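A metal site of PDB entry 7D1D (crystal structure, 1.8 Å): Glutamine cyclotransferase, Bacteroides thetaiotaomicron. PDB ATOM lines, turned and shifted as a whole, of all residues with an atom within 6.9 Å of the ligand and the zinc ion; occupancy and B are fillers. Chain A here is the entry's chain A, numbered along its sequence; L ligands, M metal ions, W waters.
The zinc ion is bound by the side-chain carboxylate (OD2) of Asp 160 (2.0 Å), the side-chain carboxylate (OD2) of Asp 127 (2.0 Å), a nitrogen (N2) of the ligand (2.0 Å), a ring nitrogen (NE2) of His 280 (2.1 Å) and the side-chain carboxylate (OD1) of Asp 160 (2.6 Å).
The zinc ion has five donor atoms within binding distance.
N1 of the ligand lies close to OE2 of Glu 159.
Merely in contact with the ligand: Asp 201 (2.8 Å), Thr 249 (3.2 Å), Trp 176 (3.5 Å), Phe 275 (3.6 Å) and Met 202 (3.97 Å).
Hydrophobic or aromatic side chains within 4 Å of the ligand: Trp 176, Met 202, Phe 275 and His 280.
Within 4 Å of the ligand: Asp 127, Glu 159, Asp 160, Trp 176, Asp 201, Met 202, Thr 249, Phe 275, Trp 279 and His 280.
The nearest printed residue that does not touch the ligand is Ile 248 (4.1 Å).
NE1 of Trp 279 sits close to N2 of the ligand (3.5 Å).
Merely in contact with the zinc ion: Trp 279.
Within 4 Å of the zinc ion: Asp 127, Asp 160, Trp 279 and His 280.
The backbone carbonyl oxygen of Asp 160 lies within hydrogen-bond range of the guanidinium group of Arg 106 (2.9 Å).
OD2 of Asp 104 lies within hydrogen-bond range of N of Asp 160, 2.9 Å away.
A ring nitrogen (NE2) of His 102 lies within hydrogen-bond range of the side-chain carboxylate (OD1) of Asp 127 (2.8 Å).
The indole nitrogen (NE1) of Trp 279 sits close to a ring nitrogen (NE2) of His 280.
ND1 of His 280 sits close to NE of Arg 106 (3.5 Å).
OD2 of Asp 201 sits close to OD2 of Asp 250, at 2.4 Å.
A ring nitrogen (NE2) of His 102 is in hydrogen-bond range of the side-chain carboxylate (OE1) of Glu 159 (3.2 Å).
The backbone NH (N) of Cys 177 sits at hydrogen-bond distance from the backbone carbonyl oxygen (O) of Glu 159 (3.1 Å).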
ATOM      1  N   HIS A 102      10.464 -19.009  -4.415  1.00  0.00           N
ATOM      2  CA  HIS A 102      11.056 -19.011  -5.762  1.00  0.00           C
ATOM      3  C   HIS A 102      10.635 -17.753  -6.523  1.00  0.00           C
ATOM      4  O   HIS A 102       9.496 -17.290  -6.391  1.00  0.00           O
ATOM      5  CB  HIS A 102      10.781 -20.297  -6.550  1.00  0.00           C
ATOM      6  CG  HIS A 102       9.500 -20.311  -7.310  1.00  0.00           C
ATOM      7  ND1 HIS A 102       9.405 -19.902  -8.622  1.00  0.00           N
ATOM      8  CD2 HIS A 102       8.266 -20.758  -6.965  1.00  0.00           C
ATOM      9  CE1 HIS A 102       8.153 -20.034  -9.040  1.00  0.00           C
ATOM     10  NE2 HIS A 102       7.444 -20.562  -8.057  1.00  0.00           N
ATOM     11  N   ASP A 104      11.745 -17.153 -10.132  1.00  0.00           N
ATOM     12  CA  ASP A 104      11.625 -17.406 -11.559  1.00  0.00           C
ATOM     13  C   ASP A 104      10.184 -17.758 -11.913  1.00  0.00           C
ATOM     14  O   ASP A 104       9.399 -18.133 -11.042  1.00  0.00           O
ATOM     15  CB  ASP A 104      12.512 -18.574 -11.966  1.00  0.00           C
ATOM     16  CG  ASP A 104      12.105 -19.892 -11.314  1.00  0.00           C
ATOM     17  OD1 ASP A 104      11.962 -19.935 -10.043  1.00  0.00           O
ATOM     18  OD2 ASP A 104      11.912 -20.873 -12.055  1.00  0.00           O
ATOM     19  N   THR A 105       9.852 -17.639 -13.184  1.00  0.00           N
ATOM     20  CA  THR A 105       8.535 -18.067 -13.642  1.00  0.00           C
ATOM     21  C   THR A 105       8.668 -19.122 -14.726  1.00  0.00           C
ATOM     22  O   THR A 105       9.693 -19.195 -15.420  1.00  0.00           O
ATOM     23  CB  THR A 105       7.647 -16.891 -14.058  1.00  0.00           C
ATOM     24  OG1 THR A 105       8.252 -16.166 -15.119  1.00  0.00           O
ATOM     25  CG2 THR A 105       7.449 -15.951 -12.908  1.00  0.00           C
ATOM     26  N   ARG A 106       7.624 -19.928 -14.870  1.00  0.00           N
ATOM     27  CA  ARG A 106       7.657 -21.094 -15.752  1.00  0.00           C
ATOM     28  C   ARG A 106       7.579 -20.692 -17.230  1.00  0.00           C
ATOM     29  O   ARG A 106       6.738 -19.888 -17.611  1.00  0.00           O
ATOM     30  CB  ARG A 106       6.514 -22.021 -15.400  1.00  0.00           C
ATOM     31  CG  ARG A 106       6.551 -23.321 -16.189  1.00  0.00           C
ATOM     32  CD  ARG A 106       5.849 -24.407 -15.432  1.00  0.00           C
ATOM     33  NE  ARG A 106       5.814 -25.687 -16.131  1.00  0.00           N
ATOM     34  CZ  ARG A 106       6.836 -26.537 -16.219  1.00  0.00           C
ATOM     35  NH1 ARG A 106       8.028 -26.261 -15.690  1.00  0.00           N
ATOM     36  NH2 ARG A 106       6.678 -27.684 -16.876  1.00  0.00           N
ATOM     37  N   ILE A 122       4.239 -18.021 -18.635  1.00  0.00           N
ATOM     38  CA  ILE A 122       3.230 -17.470 -17.741  1.00  0.00           C
ATOM     39  C   ILE A 122       3.743 -16.195 -17.071  1.00  0.00           C
ATOM     40  O   ILE A 122       4.944 -15.968 -16.985  1.00  0.00           O
ATOM     41  CB  ILE A 122       2.782 -18.495 -16.670  1.00  0.00           C
ATOM     42  CG1 ILE A 122       3.896 -18.794 -15.645  1.00  0.00           C
ATOM     43  CG2 ILE A 122       2.310 -19.793 -17.356  1.00  0.00           C
ATOM     44  CD1 ILE A 122       3.425 -19.620 -14.479  1.00  0.00           C
ATOM     45  N   ASP A 127       2.331 -17.836  -8.787  1.00  0.00           N
ATOM     46  CA  ASP A 127       3.421 -18.819  -8.842  1.00  0.00           C
ATOM     47  C   ASP A 127       4.723 -18.091  -9.191  1.00  0.00           C
ATOM     48  O   ASP A 127       5.106 -17.970 -10.360  1.00  0.00           O
ATOM     49  CB  ASP A 127       3.024 -19.869  -9.865  1.00  0.00           C
ATOM     50  CG  ASP A 127       3.977 -21.030  -9.974  1.00  0.00           C
ATOM     51  OD1 ASP A 127       4.985 -21.112  -9.233  1.00  0.00           O
ATOM     52  OD2 ASP A 127       3.689 -21.891 -10.846  1.00  0.00           O
ATOM     53  N   GLY A 128       5.388 -17.582  -8.155  1.00  0.00           N
ATOM     54  CA  GLY A 128       6.601 -16.770  -8.266  1.00  0.00           C
ATOM     55  C   GLY A 128       6.455 -15.486  -7.470  1.00  0.00           C
ATOM     56  O   GLY A 128       6.968 -15.339  -6.350  1.00  0.00           O
ATOM     57  N   GLU A 159      13.253 -22.766  -9.985  1.00  0.00           N
ATOM     58  CA  GLU A 159      12.349 -23.756  -9.406  1.00  0.00           C
ATOM     59  C   GLU A 159      11.474 -24.388 -10.470  1.00  0.00           C
ATOM     60  O   GLU A 159      11.163 -25.566 -10.368  1.00  0.00           O
ATOM     61  CB  GLU A 159      11.462 -23.142  -8.307  1.00  0.00           C
ATOM     62  CG  GLU A 159      10.454 -24.095  -7.662  1.00  0.00           C
ATOM     63  CD  GLU A 159       9.132 -24.243  -8.424  1.00  0.00           C
ATOM     64  OE1 GLU A 159       8.722 -23.298  -9.139  1.00  0.00           O
ATOM     65  OE2 GLU A 159       8.510 -25.322  -8.317  1.00  0.00           O
ATOM     66  N   ASP A 160      11.068 -23.582 -11.460  1.00  0.00           N
ATOM     67  CA  ASP A 160       9.908 -23.894 -12.292  1.00  0.00           C
ATOM     68  C   ASP A 160      10.270 -24.152 -13.756  1.00  0.00           C
ATOM     69  O   ASP A 160       9.436 -23.947 -14.658  1.00  0.00           O
ATOM     70  CB  ASP A 160       8.876 -22.745 -12.173  1.00  0.00           C
ATOM     71  CG  ASP A 160       7.459 -23.240 -11.873  1.00  0.00           C
ATOM     72  OD1 ASP A 160       7.210 -24.460 -11.812  1.00  0.00           O
ATOM     73  OD2 ASP A 160       6.570 -22.390 -11.643  1.00  0.00           O
ATOM     74  N   GLY A 162      11.140 -27.235 -14.611  1.00  0.00           N
ATOM     75  CA  GLY A 162      11.006 -28.669 -14.674  1.00  0.00           C
ATOM     76  C   GLY A 162      10.331 -29.155 -15.951  1.00  0.00           C
ATOM     77  O   GLY A 162       9.686 -28.386 -16.674  1.00  0.00           O
ATOM     78  N   TRP A 176      13.225 -30.238 -11.218  1.00  0.00           N
ATOM     79  CA  TRP A 176      12.598 -29.123 -10.509  1.00  0.00           C
ATOM     80  C   TRP A 176      13.519 -28.569  -9.452  1.00  0.00           C
ATOM     81  O   TRP A 176      14.435 -29.255  -9.014  1.00  0.00           O
ATOM     82  CB  TRP A 176      11.315 -29.600  -9.817  1.00  0.00           C
ATOM     83  CG  TRP A 176      10.315 -30.120 -10.808  1.00  0.00           C
ATOM     84  CD1 TRP A 176      10.163 -31.426 -11.220  1.00  0.00           C
ATOM     85  CD2 TRP A 176       9.366 -29.365 -11.538  1.00  0.00           C
ATOM     86  NE1 TRP A 176       9.174 -31.516 -12.166  1.00  0.00           N
ATOM     87  CE2 TRP A 176       8.657 -30.263 -12.371  1.00  0.00           C
ATOM     88  CE3 TRP A 176       9.027 -27.999 -11.578  1.00  0.00           C
ATOM     89  CZ2 TRP A 176       7.644 -29.834 -13.239  1.00  0.00           C
ATOM     90  CZ3 TRP A 176       8.017 -27.583 -12.413  1.00  0.00           C
ATOM     91  CH2 TRP A 176       7.334 -28.499 -13.246  1.00  0.00           C
ATOM     92  N   CYS A 177      13.260 -27.342  -9.009  1.00  0.00           N
ATOM     93  CA  CYS A 177      13.900 -26.826  -7.788  1.00  0.00           C
ATOM     94  C   CYS A 177      15.423 -26.842  -7.903  1.00  0.00           C
ATOM     95  O   CYS A 177      16.142 -27.262  -6.983  1.00  0.00           O
ATOM     96  CB  CYS A 177      13.454 -27.634  -6.578  1.00  0.00           C
ATOM     97  SG  CYS A 177      11.669 -27.704  -6.380  1.00  0.00           S
ATOM     98  N   ASP A 201       4.829 -20.511  -1.295  1.00  0.00           N
ATOM     99  CA  ASP A 201       4.619 -20.848  -2.698  1.00  0.00           C
ATOM    100  C   ASP A 201       3.136 -20.654  -3.013  1.00  0.00           C
ATOM    101  O   ASP A 201       2.290 -21.321  -2.429  1.00  0.00           O
ATOM    102  CB  ASP A 201       5.034 -22.293  -2.956  1.00  0.00           C
ATOM    103  CG  ASP A 201       5.118 -22.654  -4.443  1.00  0.00           C
ATOM    104  OD1 ASP A 201       4.934 -21.780  -5.338  1.00  0.00           O
ATOM    105  OD2 ASP A 201       5.396 -23.834  -4.725  1.00  0.00           O
ATOM    106  N   MET A 202       2.843 -19.724  -3.930  1.00  0.00           N
ATOM    107  CA  MET A 202       1.465 -19.396  -4.337  1.00  0.00           C
ATOM    108  C   MET A 202       0.609 -18.920  -3.155  1.00  0.00           C
ATOM    109  O   MET A 202      -0.344 -19.562  -2.766  1.00  0.00           O
ATOM    110  CB  MET A 202       0.786 -20.546  -5.081  1.00  0.00           C
ATOM    111  CG  MET A 202       1.470 -20.870  -6.404  1.00  0.00           C
ATOM    112  SD  MET A 202       0.754 -22.249  -7.292  1.00  0.00           S
ATOM    113  CE  MET A 202       1.505 -23.586  -6.365  1.00  0.00           C
ATOM    114  N   ILE A 248       3.700 -32.533  -1.837  1.00  0.00           N
ATOM    115  CA  ILE A 248       4.055 -31.716  -2.999  1.00  0.00           C
ATOM    116  C   ILE A 248       5.568 -31.620  -3.167  1.00  0.00           C
ATOM    117  O   ILE A 248       6.272 -31.199  -2.249  1.00  0.00           O
ATOM    118  CB  ILE A 248       3.491 -30.265  -2.867  1.00  0.00           C
ATOM    119  CG1 ILE A 248       1.959 -30.285  -2.736  1.00  0.00           C
ATOM    120  CG2 ILE A 248       3.908 -29.410  -4.044  1.00  0.00           C
ATOM    121  CD1 ILE A 248       1.211 -30.923  -3.898  1.00  0.00           C
ATOM    122  N   THR A 249       6.051 -31.991  -4.348  1.00  0.00           N
ATOM    123  CA  THR A 249       7.443 -31.751  -4.702  1.00  0.00           C
ATOM    124  C   THR A 249       7.635 -30.240  -4.839  1.00  0.00           C
ATOM    125  O   THR A 249       7.012 -29.598  -5.678  1.00  0.00           O
ATOM    126  CB  THR A 249       7.837 -32.430  -6.020  1.00  0.00           C
ATOM    127  OG1 THR A 249       7.581 -33.835  -5.916  1.00  0.00           O
ATOM    128  CG2 THR A 249       9.308 -32.220  -6.331  1.00  0.00           C
ATOM    129  N   ASP A 250       8.464 -29.675  -3.972  1.00  0.00           N
ATOM    130  CA  ASP A 250       8.691 -28.236  -3.967  1.00  0.00           C
ATOM    131  C   ASP A 250      10.076 -28.017  -3.360  1.00  0.00           C
ATOM    132  O   ASP A 250      10.735 -28.989  -2.932  1.00  0.00           O
ATOM    133  CB  ASP A 250       7.556 -27.540  -3.173  1.00  0.00           C
ATOM    134  CG  ASP A 250       7.269 -26.124  -3.665  1.00  0.00           C
ATOM    135  OD1 ASP A 250       8.052 -25.591  -4.476  1.00  0.00           O
ATOM    136  OD2 ASP A 250       6.249 -25.539  -3.197  1.00  0.00           O
ATOM    137  N   ASP A 251      10.516 -26.762  -3.318  1.00  0.00           N
ATOM    138  CA  ASP A 251      11.892 -26.454  -2.851  1.00  0.00           C
ATOM    139  C   ASP A 251      12.231 -26.991  -1.466  1.00  0.00           C
ATOM    140  O   ASP A 251      13.385 -27.353  -1.175  1.00  0.00           O
ATOM    141  CB  ASP A 251      12.127 -24.942  -2.852  1.00  0.00           C
ATOM    142  CG  ASP A 251      12.142 -24.333  -4.239  1.00  0.00           C
ATOM    143  OD1 ASP A 251      12.947 -24.769  -5.093  1.00  0.00           O
ATOM    144  OD2 ASP A 251      11.355 -23.383  -4.449  1.00  0.00           O
ATOM    145  N   ASP A 265       6.292 -25.973   3.880  1.00  0.00           N
ATOM    146  CA  ASP A 265       5.781 -25.293   2.688  1.00  0.00           C
ATOM    147  C   ASP A 265       4.386 -24.770   3.020  1.00  0.00           C
ATOM    148  O   ASP A 265       3.528 -25.525   3.519  1.00  0.00           O
ATOM    149  CB  ASP A 265       5.710 -26.313   1.542  1.00  0.00           C
ATOM    150  CG  ASP A 265       5.553 -25.671   0.150  1.00  0.00           C
ATOM    151  OD1 ASP A 265       5.554 -24.431   0.008  1.00  0.00           O
ATOM    152  OD2 ASP A 265       5.435 -26.453  -0.822  1.00  0.00           O
ATOM    153  N   ILE A 267       1.507 -23.578   0.985  1.00  0.00           N
ATOM    154  CA  ILE A 267       1.094 -23.758  -0.397  1.00  0.00           C
ATOM    155  C   ILE A 267      -0.411 -24.077  -0.408  1.00  0.00           C
ATOM    156  O   ILE A 267      -0.870 -24.785   0.486  1.00  0.00           O
ATOM    157  CB  ILE A 267       1.943 -24.856  -1.089  1.00  0.00           C
ATOM    158  CG1 ILE A 267       1.674 -24.881  -2.589  1.00  0.00           C
ATOM    159  CG2 ILE A 267       1.749 -26.237  -0.459  1.00  0.00           C
ATOM    160  CD1 ILE A 267       2.718 -25.632  -3.369  1.00  0.00           C
ATOM    161  N   PHE A 275      -4.096 -27.300  -6.719  1.00  0.00           N
ATOM    162  CA  PHE A 275      -3.534 -25.958  -6.774  1.00  0.00           C
ATOM    163  C   PHE A 275      -4.600 -24.980  -7.251  1.00  0.00           C
ATOM    164  O   PHE A 275      -5.645 -25.406  -7.747  1.00  0.00           O
ATOM    165  CB  PHE A 275      -2.333 -25.918  -7.725  1.00  0.00           C
ATOM    166  CG  PHE A 275      -1.128 -26.669  -7.235  1.00  0.00           C
ATOM    167  CD1 PHE A 275      -0.804 -26.760  -5.879  1.00  0.00           C
ATOM    168  CD2 PHE A 275      -0.273 -27.242  -8.161  1.00  0.00           C
ATOM    169  CE1 PHE A 275       0.321 -27.445  -5.462  1.00  0.00           C
ATOM    170  CE2 PHE A 275       0.865 -27.925  -7.739  1.00  0.00           C
ATOM    171  CZ  PHE A 275       1.156 -28.013  -6.397  1.00  0.00           C
ATOM    172  N   TRP A 279      -2.917 -22.189 -11.991  1.00  0.00           N
ATOM    173  CA  TRP A 279      -1.584 -22.822 -11.974  1.00  0.00           C
ATOM    174  C   TRP A 279      -1.134 -23.330 -13.358  1.00  0.00           C
ATOM    175  O   TRP A 279      -1.821 -24.136 -13.982  1.00  0.00           O
ATOM    176  CB  TRP A 279      -1.582 -23.985 -11.004  1.00  0.00           C
ATOM    177  CG  TRP A 279      -0.287 -24.722 -10.898  1.00  0.00           C
ATOM    178  CD1 TRP A 279       0.819 -24.327 -10.205  1.00  0.00           C
ATOM    179  CD2 TRP A 279       0.019 -25.995 -11.454  1.00  0.00           C
ATOM    180  NE1 TRP A 279       1.803 -25.290 -10.292  1.00  0.00           N
ATOM    181  CE2 TRP A 279       1.339 -26.331 -11.050  1.00  0.00           C
ATOM    182  CE3 TRP A 279      -0.692 -26.914 -12.256  1.00  0.00           C
ATOM    183  CZ2 TRP A 279       1.952 -27.536 -11.421  1.00  0.00           C
ATOM    184  CZ3 TRP A 279      -0.086 -28.092 -12.618  1.00  0.00           C
ATOM    185  CH2 TRP A 279       1.239 -28.392 -12.221  1.00  0.00           C
ATOM    186  N   HIS A 280       0.007 -22.819 -13.816  1.00  0.00           N
ATOM    187  CA  HIS A 280       0.612 -23.176 -15.108  1.00  0.00           C
ATOM    188  C   HIS A 280      -0.328 -22.962 -16.313  1.00  0.00           C
ATOM    189  O   HIS A 280      -0.290 -23.722 -17.295  1.00  0.00           O
ATOM    190  CB  HIS A 280       1.221 -24.589 -15.067  1.00  0.00           C
ATOM    191  CG  HIS A 280       2.359 -24.693 -14.111  1.00  0.00           C
ATOM    192  ND1 HIS A 280       3.105 -25.835 -13.958  1.00  0.00           N
ATOM    193  CD2 HIS A 280       2.889 -23.776 -13.265  1.00  0.00           C
ATOM    194  CE1 HIS A 280       4.050 -25.624 -13.057  1.00  0.00           C
ATOM    195  NE2 HIS A 280       3.920 -24.385 -12.614  1.00  0.00           N
ATOM    196  N   ASP A 284      -2.368 -16.927 -14.799  1.00  0.00           N
ATOM    197  CA  ASP A 284      -1.685 -16.626 -13.549  1.00  0.00           C
ATOM    198  C   ASP A 284      -1.152 -15.202 -13.602  1.00  0.00           C
ATOM    199  O   ASP A 284       0.050 -14.972 -13.796  1.00  0.00           O
ATOM    200  CB  ASP A 284      -0.592 -17.653 -13.247  1.00  0.00           C
ATOM    201  CG  ASP A 284       0.015 -17.446 -11.858  1.00  0.00           C
ATOM    202  OD1 ASP A 284      -0.454 -16.557 -11.094  1.00  0.00           O
ATOM    203  OD2 ASP A 284       0.967 -18.164 -11.515  1.00  0.00           O
HETATM  204  C1  LIG L   1       5.139 -24.902  -7.284  1.00  0.00           C
HETATM  205  C2  LIG L   1       5.019 -23.948  -8.214  1.00  0.00           C
HETATM  206  N1  LIG L   1       5.237 -26.048  -7.943  1.00  0.00           N
HETATM  207  C3  LIG L   1       5.192 -25.825  -9.253  1.00  0.00           C
HETATM  208  N2  LIG L   1       5.057 -24.518  -9.426  1.00  0.00           N
HETATM  209  C4  LIG L   1       5.391 -27.344  -7.230  1.00  0.00           C
HETATM  210  C5  LIG L   1       5.317 -28.576  -8.148  1.00  0.00           C
HETATM  211  C6  LIG L   1       4.180 -29.378  -8.147  1.00  0.00           C
HETATM  212  C7  LIG L   1       6.382 -28.881  -8.987  1.00  0.00           C
HETATM  213  C8  LIG L   1       4.111 -30.487  -8.992  1.00  0.00           C
HETATM  214  C9  LIG L   1       6.327 -29.988  -9.827  1.00  0.00           C
HETATM  215  C10 LIG L   1       5.184 -30.799  -9.828  1.00  0.00           C
HETATM  216 ZN    ZN M   1       4.959 -23.373 -11.098  1.00  0.00          ZN
HETATM  217  O   HOH W   1       4.177 -32.248  -6.645  1.00  0.00           O
